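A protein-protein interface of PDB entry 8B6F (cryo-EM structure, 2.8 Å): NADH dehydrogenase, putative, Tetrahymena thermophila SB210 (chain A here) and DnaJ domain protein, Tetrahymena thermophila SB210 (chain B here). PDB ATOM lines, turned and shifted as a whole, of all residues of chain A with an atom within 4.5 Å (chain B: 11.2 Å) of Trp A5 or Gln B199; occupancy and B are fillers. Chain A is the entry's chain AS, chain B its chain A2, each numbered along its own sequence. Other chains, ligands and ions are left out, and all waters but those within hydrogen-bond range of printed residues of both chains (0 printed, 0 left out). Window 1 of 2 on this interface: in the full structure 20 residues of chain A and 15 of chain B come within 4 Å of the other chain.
The side-chain amide nitrogen of Gln B199 sits at hydrogen-bond distance from the backbone carbonyl oxygen of Trp A5, at 3.0 Å.
The backbone carbonyl oxygen (O) of Tyr A4 is in hydrogen-bond range of the side-chain amide nitrogen (ND2) of Asn A28 (3.3 Å). The side-chain carboxylate (OD1) of Asp B194 is in hydrogen-bond range of the side-chain hydroxyl (OG1) of Thr B195 (2.9 Å). The backbone NH of Trp A5 lies close to a ring nitrogen (ND1) of His A3, 3.2 Å away. The backbone carbonyl oxygen of Gly A6 sits at hydrogen-bond distance from the side-chain amide nitrogen of Asn A28, at 3.3 Å.
Among the printed residues, merely in contact across the chains: His A3 with Asp B194 (3.3 Å), His A3 with Met B196 (3.5 Å), Trp A5 with Met B196 (3.5 Å), Trp A5 with Asp B197 (3.6 Å), Trp A5 with Tyr B198 (3.7 Å), Asn A28 with Gln B199 (3.6 Å), Val A29 with Gln B199 (3.9 Å), Val A29 with Ile B201 (3.5 Å), Lys A62 with Gln B199 (3.0 Å), Tyr A113 with Asp B197 (3.5 Å) and Tyr A113 with Tyr B198 (3.5 Å).
Printed residues of chain B within 4 Å of Trp A5: Met B196 (3.5 Å), Asp B197 (3.6 Å), Tyr B198 (3.7 Å) and Gln B199 (3.0 Å). Of chain A, only Trp A5, Asn A28, Val A29 and Lys A62 come within 4 Å of Gln B199. No residue of chain B comes within 4 Å of Ser A7. Printed residues of chain A within 4 Å of Tyr B198: Trp A5 and Tyr A113. Printed residues of chain A within 4 Å of Asp B194: His A3 (3.3 Å). Of the printed residues of chain A, Met B196 touches His A3 (3.5 Å) and Trp A5 (3.5 Å). Printed residues of chain A within 4 Å of Ile B201: Val A29 (3.5 Å). Of the printed residues of chain A, Asp B197 touches Trp A5 and Tyr A113. Thr B202 touches none of the printed residues of chain A. Gly A6 touches none of the printed residues of chain B. The nearest printed residue of chain A that does not touch Gln B199 is Gly A6 (4.8 Å).
Of the 19 printed residues of chain B, 6 touch a printed residue of chain A. Among the printed residues, no Asp or Glu carboxylate lies within 4 Å of a Lys or Arg side-chain nitrogen of the other chain.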
ATOM      1  N   HIS A   3      19.501  16.422 -25.913  1.00  0.00           N
ATOM      2  CA  HIS A   3      19.651  15.162 -26.623  1.00  0.00           C
ATOM      3  C   HIS A   3      18.770  14.129 -25.941  1.00  0.00           C
ATOM      4  O   HIS A   3      18.374  14.294 -24.785  1.00  0.00           O
ATOM      5  CB  HIS A   3      21.115  14.708 -26.637  1.00  0.00           C
ATOM      6  CG  HIS A   3      21.416  13.658 -27.660  1.00  0.00           C
ATOM      7  ND1 HIS A   3      21.152  12.321 -27.457  1.00  0.00           N
ATOM      8  CD2 HIS A   3      21.973  13.748 -28.890  1.00  0.00           C
ATOM      9  CE1 HIS A   3      21.526  11.634 -28.521  1.00  0.00           C
ATOM     10  NE2 HIS A   3      22.029  12.476 -29.405  1.00  0.00           N
ATOM     11  N   TYR A   4      18.457  13.058 -26.670  1.00  0.00           N
ATOM     12  CA  TYR A   4      17.613  12.014 -26.098  1.00  0.00           C
ATOM     13  C   TYR A   4      18.276  11.354 -24.896  1.00  0.00           C
ATOM     14  O   TYR A   4      17.584  10.905 -23.976  1.00  0.00           O
ATOM     15  CB  TYR A   4      17.278  10.967 -27.158  1.00  0.00           C
ATOM     16  CG  TYR A   4      16.432   9.838 -26.627  1.00  0.00           C
ATOM     17  CD1 TYR A   4      15.086  10.027 -26.348  1.00  0.00           C
ATOM     18  CD2 TYR A   4      16.977   8.583 -26.407  1.00  0.00           C
ATOM     19  CE1 TYR A   4      14.308   8.997 -25.861  1.00  0.00           C
ATOM     20  CE2 TYR A   4      16.208   7.547 -25.921  1.00  0.00           C
ATOM     21  CZ  TYR A   4      14.874   7.760 -25.650  1.00  0.00           C
ATOM     22  OH  TYR A   4      14.106   6.731 -25.165  1.00  0.00           O
ATOM     23  N   TRP A   5      19.602  11.285 -24.884  1.00  0.00           N
ATOM     24  CA  TRP A   5      20.356  10.689 -23.793  1.00  0.00           C
ATOM     25  C   TRP A   5      20.763  11.704 -22.733  1.00  0.00           C
ATOM     26  O   TRP A   5      21.494  11.350 -21.804  1.00  0.00           O
ATOM     27  CB  TRP A   5      21.602   9.994 -24.342  1.00  0.00           C
ATOM     28  CG  TRP A   5      21.300   8.809 -25.202  1.00  0.00           C
ATOM     29  CD1 TRP A   5      20.253   7.945 -25.070  1.00  0.00           C
ATOM     30  CD2 TRP A   5      22.052   8.358 -26.333  1.00  0.00           C
ATOM     31  NE1 TRP A   5      20.308   6.983 -26.046  1.00  0.00           N
ATOM     32  CE2 TRP A   5      21.405   7.213 -26.833  1.00  0.00           C
ATOM     33  CE3 TRP A   5      23.214   8.809 -26.967  1.00  0.00           C
ATOM     34  CZ2 TRP A   5      21.877   6.515 -27.941  1.00  0.00           C
ATOM     35  CZ3 TRP A   5      23.682   8.114 -28.065  1.00  0.00           C
ATOM     36  CH2 TRP A   5      23.015   6.979 -28.542  1.00  0.00           C
ATOM     37  N   GLY A   6      20.311  12.949 -22.851  1.00  0.00           N
ATOM     38  CA  GLY A   6      20.698  13.957 -21.886  1.00  0.00           C
ATOM     39  C   GLY A   6      20.200  13.623 -20.493  1.00  0.00           C
ATOM     40  O   GLY A   6      19.205  12.922 -20.311  1.00  0.00           O
ATOM     41  N   SER A   7      20.912  14.144 -19.494  1.00  0.00           N
ATOM     42  CA  SER A   7      20.571  13.879 -18.103  1.00  0.00           C
ATOM     43  C   SER A   7      19.245  14.502 -17.690  1.00  0.00           C
ATOM     44  O   SER A   7      18.722  14.146 -16.628  1.00  0.00           O
ATOM     45  CB  SER A   7      21.685  14.385 -17.187  1.00  0.00           C
ATOM     46  OG  SER A   7      21.916  15.769 -17.379  1.00  0.00           O
ATOM     47  N   ASN A  28      17.587   7.110 -16.860  1.00  0.00           N
ATOM     48  CA  ASN A  28      17.478   7.194 -18.308  1.00  0.00           C
ATOM     49  C   ASN A  28      18.407   6.220 -19.014  1.00  0.00           C
ATOM     50  O   ASN A  28      18.426   6.199 -20.248  1.00  0.00           O
ATOM     51  CB  ASN A  28      17.779   8.629 -18.774  1.00  0.00           C
ATOM     52  CG  ASN A  28      17.379   8.876 -20.209  1.00  0.00           C
ATOM     53  OD1 ASN A  28      16.616   8.110 -20.796  1.00  0.00           O
ATOM     54  ND2 ASN A  28      17.884   9.961 -20.782  1.00  0.00           N
ATOM     55  N   VAL A  29      19.170   5.416 -18.277  1.00  0.00           N
ATOM     56  CA  VAL A  29      20.124   4.492 -18.876  1.00  0.00           C
ATOM     57  C   VAL A  29      19.511   3.115 -19.082  1.00  0.00           C
ATOM     58  O   VAL A  29      19.707   2.495 -20.129  1.00  0.00           O
ATOM     59  CB  VAL A  29      21.389   4.420 -17.996  1.00  0.00           C
ATOM     60  CG1 VAL A  29      22.393   3.441 -18.575  1.00  0.00           C
ATOM     61  CG2 VAL A  29      22.009   5.798 -17.847  1.00  0.00           C
ATOM     62  N   LYS A  62      25.753  -0.041 -23.809  1.00  0.00           N
ATOM     63  CA  LYS A  62      24.396   0.486 -23.746  1.00  0.00           C
ATOM     64  C   LYS A  62      23.375  -0.613 -24.003  1.00  0.00           C
ATOM     65  O   LYS A  62      22.345  -0.685 -23.324  1.00  0.00           O
ATOM     66  CB  LYS A  62      24.230   1.621 -24.758  1.00  0.00           C
ATOM     67  CG  LYS A  62      22.937   2.408 -24.614  1.00  0.00           C
ATOM     68  CD  LYS A  62      22.834   3.035 -23.231  1.00  0.00           C
ATOM     69  CE  LYS A  62      21.773   4.116 -23.171  1.00  0.00           C
ATOM     70  NZ  LYS A  62      20.440   3.634 -23.599  1.00  0.00           N
ATOM     71  N   TYR A 113      22.412   1.791 -32.850  1.00  0.00           N
ATOM     72  CA  TYR A 113      21.708   2.683 -31.935  1.00  0.00           C
ATOM     73  C   TYR A 113      20.269   2.895 -32.379  1.00  0.00           C
ATOM     74  O   TYR A 113      19.354   2.925 -31.550  1.00  0.00           O
ATOM     75  CB  TYR A 113      22.437   4.023 -31.847  1.00  0.00           C
ATOM     76  CG  TYR A 113      23.582   4.053 -30.861  1.00  0.00           C
ATOM     77  CD1 TYR A 113      23.434   3.558 -29.571  1.00  0.00           C
ATOM     78  CD2 TYR A 113      24.812   4.583 -31.221  1.00  0.00           C
ATOM     79  CE1 TYR A 113      24.480   3.591 -28.671  1.00  0.00           C
ATOM     80  CE2 TYR A 113      25.861   4.620 -30.329  1.00  0.00           C
ATOM     81  CZ  TYR A 113      25.690   4.122 -29.057  1.00  0.00           C
ATOM     82  OH  TYR A 113      26.737   4.159 -28.170  1.00  0.00           O
ATOM     83  N   LEU B 185      29.608  19.906 -17.761  1.00  0.00           N
ATOM     84  CA  LEU B 185      28.364  19.773 -18.515  1.00  0.00           C
ATOM     85  C   LEU B 185      28.105  21.005 -19.372  1.00  0.00           C
ATOM     86  O   LEU B 185      27.683  20.886 -20.528  1.00  0.00           O
ATOM     87  CB  LEU B 185      27.192  19.526 -17.565  1.00  0.00           C
ATOM     88  CG  LEU B 185      25.820  19.384 -18.233  1.00  0.00           C
ATOM     89  CD1 LEU B 185      25.831  18.286 -19.286  1.00  0.00           C
ATOM     90  CD2 LEU B 185      24.742  19.113 -17.200  1.00  0.00           C
ATOM     91  N   GLN B 188      30.413  20.880 -22.320  1.00  0.00           N
ATOM     92  CA  GLN B 188      29.943  19.940 -23.330  1.00  0.00           C
ATOM     93  C   GLN B 188      28.765  20.512 -24.107  1.00  0.00           C
ATOM     94  O   GLN B 188      28.693  20.370 -25.332  1.00  0.00           O
ATOM     95  CB  GLN B 188      29.557  18.616 -22.672  1.00  0.00           C
ATOM     96  CG  GLN B 188      29.158  17.533 -23.658  1.00  0.00           C
ATOM     97  CD  GLN B 188      28.677  16.272 -22.971  1.00  0.00           C
ATOM     98  OE1 GLN B 188      28.516  16.239 -21.752  1.00  0.00           O
ATOM     99  NE2 GLN B 188      28.444  15.225 -23.754  1.00  0.00           N
ATOM    100  N   ILE B 189      27.825  21.154 -23.411  1.00  0.00           N
ATOM    101  CA  ILE B 189      26.671  21.737 -24.092  1.00  0.00           C
ATOM    102  C   ILE B 189      27.121  22.796 -25.089  1.00  0.00           C
ATOM    103  O   ILE B 189      26.617  22.863 -26.215  1.00  0.00           O
ATOM    104  CB  ILE B 189      25.681  22.313 -23.060  1.00  0.00           C
ATOM    105  CG1 ILE B 189      24.994  21.176 -22.301  1.00  0.00           C
ATOM    106  CG2 ILE B 189      24.642  23.202 -23.739  1.00  0.00           C
ATOM    107  CD1 ILE B 189      24.133  21.639 -21.142  1.00  0.00           C
ATOM    108  N   SER B 192      29.694  20.834 -27.978  1.00  0.00           N
ATOM    109  CA  SER B 192      29.072  19.759 -28.742  1.00  0.00           C
ATOM    110  C   SER B 192      27.556  19.834 -28.641  1.00  0.00           C
ATOM    111  O   SER B 192      26.878  18.825 -28.440  1.00  0.00           O
ATOM    112  CB  SER B 192      29.565  18.395 -28.266  1.00  0.00           C
ATOM    113  OG  SER B 192      30.968  18.272 -28.422  1.00  0.00           O
ATOM    114  N   ASP B 194      23.862  19.558 -28.965  1.00  0.00           N
ATOM    115  CA  ASP B 194      22.914  18.660 -29.622  1.00  0.00           C
ATOM    116  C   ASP B 194      23.544  17.345 -30.069  1.00  0.00           C
ATOM    117  O   ASP B 194      22.813  16.472 -30.543  1.00  0.00           O
ATOM    118  CB  ASP B 194      22.227  19.318 -30.832  1.00  0.00           C
ATOM    119  CG  ASP B 194      22.743  18.802 -32.165  1.00  0.00           C
ATOM    120  OD1 ASP B 194      23.970  18.799 -32.389  1.00  0.00           O
ATOM    121  OD2 ASP B 194      21.909  18.397 -33.002  1.00  0.00           O
ATOM    122  N   THR B 195      24.853  17.160 -29.925  1.00  0.00           N
ATOM    123  CA  THR B 195      25.538  15.962 -30.395  1.00  0.00           C
ATOM    124  C   THR B 195      26.007  15.130 -29.209  1.00  0.00           C
ATOM    125  O   THR B 195      26.680  15.645 -28.312  1.00  0.00           O
ATOM    126  CB  THR B 195      26.732  16.328 -31.279  1.00  0.00           C
ATOM    127  OG1 THR B 195      26.279  17.083 -32.410  1.00  0.00           O
ATOM    128  CG2 THR B 195      27.449  15.077 -31.771  1.00  0.00           C
ATOM    129  N   MET B 196      25.647  13.848 -29.212  1.00  0.00           N
ATOM    130  CA  MET B 196      26.105  12.896 -28.202  1.00  0.00           C
ATOM    131  C   MET B 196      26.411  11.581 -28.902  1.00  0.00           C
ATOM    132  O   MET B 196      25.493  10.886 -29.344  1.00  0.00           O
ATOM    133  CB  MET B 196      25.060  12.690 -27.106  1.00  0.00           C
ATOM    134  CG  MET B 196      24.949  13.842 -26.123  1.00  0.00           C
ATOM    135  SD  MET B 196      23.789  13.513 -24.781  1.00  0.00           S
ATOM    136  CE  MET B 196      24.584  12.141 -23.951  1.00  0.00           C
ATOM    137  N   ASP B 197      27.697  11.243 -29.007  1.00  0.00           N
ATOM    138  CA  ASP B 197      28.071   9.967 -29.608  1.00  0.00           C
ATOM    139  C   ASP B 197      27.536   8.799 -28.790  1.00  0.00           C
ATOM    140  O   ASP B 197      27.061   7.804 -29.348  1.00  0.00           O
ATOM    141  CB  ASP B 197      29.591   9.875 -29.740  1.00  0.00           C
ATOM    142  CG  ASP B 197      30.155  10.920 -30.674  1.00  0.00           C
ATOM    143  OD1 ASP B 197      29.419  11.372 -31.574  1.00  0.00           O
ATOM    144  OD2 ASP B 197      31.336  11.289 -30.513  1.00  0.00           O
ATOM    145  N   TYR B 198      27.611   8.903 -27.467  1.00  0.00           N
ATOM    146  CA  TYR B 198      27.107   7.870 -26.577  1.00  0.00           C
ATOM    147  C   TYR B 198      26.675   8.532 -25.279  1.00  0.00           C
ATOM    148  O   TYR B 198      27.093   9.648 -24.963  1.00  0.00           O
ATOM    149  CB  TYR B 198      28.164   6.793 -26.310  1.00  0.00           C
ATOM    150  CG  TYR B 198      29.360   7.303 -25.544  1.00  0.00           C
ATOM    151  CD1 TYR B 198      30.320   8.092 -26.162  1.00  0.00           C
ATOM    152  CD2 TYR B 198      29.531   6.992 -24.203  1.00  0.00           C
ATOM    153  CE1 TYR B 198      31.414   8.561 -25.464  1.00  0.00           C
ATOM    154  CE2 TYR B 198      30.620   7.457 -23.497  1.00  0.00           C
ATOM    155  CZ  TYR B 198      31.558   8.240 -24.132  1.00  0.00           C
ATOM    156  OH  TYR B 198      32.646   8.701 -23.431  1.00  0.00           O
ATOM    157  N   GLN B 199      25.819   7.839 -24.533  1.00  0.00           N
ATOM    158  CA  GLN B 199      25.357   8.342 -23.241  1.00  0.00           C
ATOM    159  C   GLN B 199      26.454   8.081 -22.220  1.00  0.00           C
ATOM    160  O   GLN B 199      26.462   7.063 -21.528  1.00  0.00           O
ATOM    161  CB  GLN B 199      24.045   7.687 -22.834  1.00  0.00           C
ATOM    162  CG  GLN B 199      23.459   8.271 -21.557  1.00  0.00           C
ATOM    163  CD  GLN B 199      22.060   7.775 -21.266  1.00  0.00           C
ATOM    164  OE1 GLN B 199      21.690   6.669 -21.646  1.00  0.00           O
ATOM    165  NE2 GLN B 199      21.272   8.599 -20.589  1.00  0.00           N
ATOM    166  N   ASN B 200      27.398   9.013 -22.127  1.00  0.00           N
ATOM    167  CA  ASN B 200      28.493   8.870 -21.179  1.00  0.00           C
ATOM    168  C   ASN B 200      27.959   8.947 -19.755  1.00  0.00           C
ATOM    169  O   ASN B 200      27.171   9.836 -19.422  1.00  0.00           O
ATOM    170  CB  ASN B 200      29.545   9.952 -21.413  1.00  0.00           C
ATOM    171  CG  ASN B 200      29.002  11.347 -21.208  1.00  0.00           C
ATOM    172  OD1 ASN B 200      27.806  11.588 -21.354  1.00  0.00           O
ATOM    173  ND2 ASN B 200      29.881  12.278 -20.865  1.00  0.00           N
ATOM    174  N   ILE B 201      28.386   8.006 -18.917  1.00  0.00           N
ATOM    175  CA  ILE B 201      27.949   7.940 -17.527  1.00  0.00           C
ATOM    176  C   ILE B 201      28.975   8.699 -16.692  1.00  0.00           C
ATOM    177  O   ILE B 201      30.009   8.154 -16.305  1.00  0.00           O
ATOM    178  CB  ILE B 201      27.788   6.496 -17.051  1.00  0.00           C
ATOM    179  CG1 ILE B 201      26.826   5.729 -17.964  1.00  0.00           C
ATOM    180  CG2 ILE B 201      27.288   6.459 -15.615  1.00  0.00           C
ATOM    181  CD1 ILE B 201      25.456   6.360 -18.110  1.00  0.00           C
ATOM    182  N   THR B 202      28.690   9.968 -16.422  1.00  0.00           N
ATOM    183  CA  THR B 202      29.526  10.768 -15.545  1.00  0.00           C
ATOM    184  C   THR B 202      29.140  10.517 -14.089  1.00  0.00           C
ATOM    185  O   THR B 202      28.208   9.769 -13.785  1.00  0.00           O
ATOM    186  CB  THR B 202      29.401  12.250 -15.897  1.00  0.00           C
ATOM    187  OG1 THR B 202      28.028  12.650 -15.807  1.00  0.00           O
ATOM    188  CG2 THR B 202      29.910  12.509 -17.301  1.00  0.00           C
ATOM    189  N   ASN B 203      29.870  11.150 -13.170  1.00  0.00           N
ATOM    190  CA  ASN B 203      29.517  11.044 -11.758  1.00  0.00           C
ATOM    191  C   ASN B 203      28.122  11.599 -11.503  1.00  0.00           C
ATOM    192  O   ASN B 203      27.364  11.047 -10.699  1.00  0.00           O
ATOM    193  CB  ASN B 203      30.548  11.778 -10.900  1.00  0.00           C
ATOM    194  CG  ASN B 203      31.874  11.054 -10.837  1.00  0.00           C
ATOM    195  OD1 ASN B 203      32.243  10.329 -11.759  1.00  0.00           O
ATOM    196  ND2 ASN B 203      32.599  11.245  -9.745  1.00  0.00           N
ATOM    197  N   GLU B 204      27.770  12.697 -12.172  1.00  0.00           N
ATOM    198  CA  GLU B 204      26.434  13.259 -12.008  1.00  0.00           C
ATOM    199  C   GLU B 204      25.364  12.283 -12.474  1.00  0.00           C
ATOM    200  O   GLU B 204      24.340  12.106 -11.806  1.00  0.00           O
ATOM    201  CB  GLU B 204      26.326  14.574 -12.779  1.00  0.00           C
ATOM    202  CG  GLU B 204      24.970  15.247 -12.661  1.00  0.00           C
ATOM    203  CD  GLU B 204      24.878  16.505 -13.494  1.00  0.00           C
ATOM    204  OE1 GLU B 204      25.919  16.942 -14.027  1.00  0.00           O
ATOM    205  OE2 GLU B 204      23.764  17.055 -13.620  1.00  0.00           O
ATOM    206  N   VAL B 205      25.575  11.645 -13.627  1.00  0.00           N
ATOM    207  CA  VAL B 205      24.590  10.694 -14.135  1.00  0.00           C
ATOM    208  C   VAL B 205      24.478   9.501 -13.199  1.00  0.00           C
ATOM    209  O   VAL B 205      23.375   9.026 -12.903  1.00  0.00           O
ATOM    210  CB  VAL B 205      24.953  10.257 -15.566  1.00  0.00           C
ATOM    211  CG1 VAL B 205      23.983   9.198 -16.069  1.00  0.00           C
ATOM    212  CG2 VAL B 205      24.960  11.453 -16.497  1.00  0.00           C
ATOM    213  N   ALA B 206      25.614   8.992 -12.724  1.00  0.00           N
ATOM    214  CA  ALA B 206      25.583   7.861 -11.805  1.00  0.00           C
ATOM    215  C   ALA B 206      24.859   8.223 -10.517  1.00  0.00           C
ATOM    216  O   ALA B 206      24.076   7.425  -9.989  1.00  0.00           O
ATOM    217  CB  ALA B 206      27.006   7.390 -11.506  1.00  0.00           C
ATOM    218  N   ASN B 208      22.561  10.573 -10.146  1.00  0.00           N
ATOM    219  CA  ASN B 208      21.139  10.695 -10.448  1.00  0.00           C
ATOM    220  C   ASN B 208      20.477   9.326 -10.493  1.00  0.00           C
ATOM    221  O   ASN B 208      19.367   9.148  -9.979  1.00  0.00           O
ATOM    222  CB  ASN B 208      20.938  11.428 -11.773  1.00  0.00           C
ATOM    223  CG  ASN B 208      21.436  12.856 -11.732  1.00  0.00           C
ATOM    224  OD1 ASN B 208      21.551  13.457 -10.665  1.00  0.00           O
ATOM    225  ND2 ASN B 208      21.722  13.414 -12.901  1.00  0.00           N
ATOM    226  N   PHE B 209      21.136   8.349 -11.117  1.00  0.00           N
ATOM    227  CA  PHE B 209      20.600   6.994 -11.138  1.00  0.00           C
ATOM    228  C   PHE B 209      20.461   6.444  -9.726  1.00  0.00           C
ATOM    229  O   PHE B 209      19.432   5.853  -9.378  1.00  0.00           O
ATOM    230  CB  PHE B 209      21.503   6.094 -11.982  1.00  0.00           C
ATOM    231  CG  PHE B 209      20.983   4.695 -12.152  1.00  0.00           C
ATOM    232  CD1 PHE B 209      21.250   3.721 -11.205  1.00  0.00           C
ATOM    233  CD2 PHE B 209      20.244   4.350 -13.270  1.00  0.00           C
ATOM    234  CE1 PHE B 209      20.779   2.433 -11.363  1.00  0.00           C
ATOM    235  CE2 PHE B 209      19.770   3.063 -13.433  1.00  0.00           C
ATOM    236  CZ  PHE B 209      20.037   2.104 -12.477  1.00  0.00           C
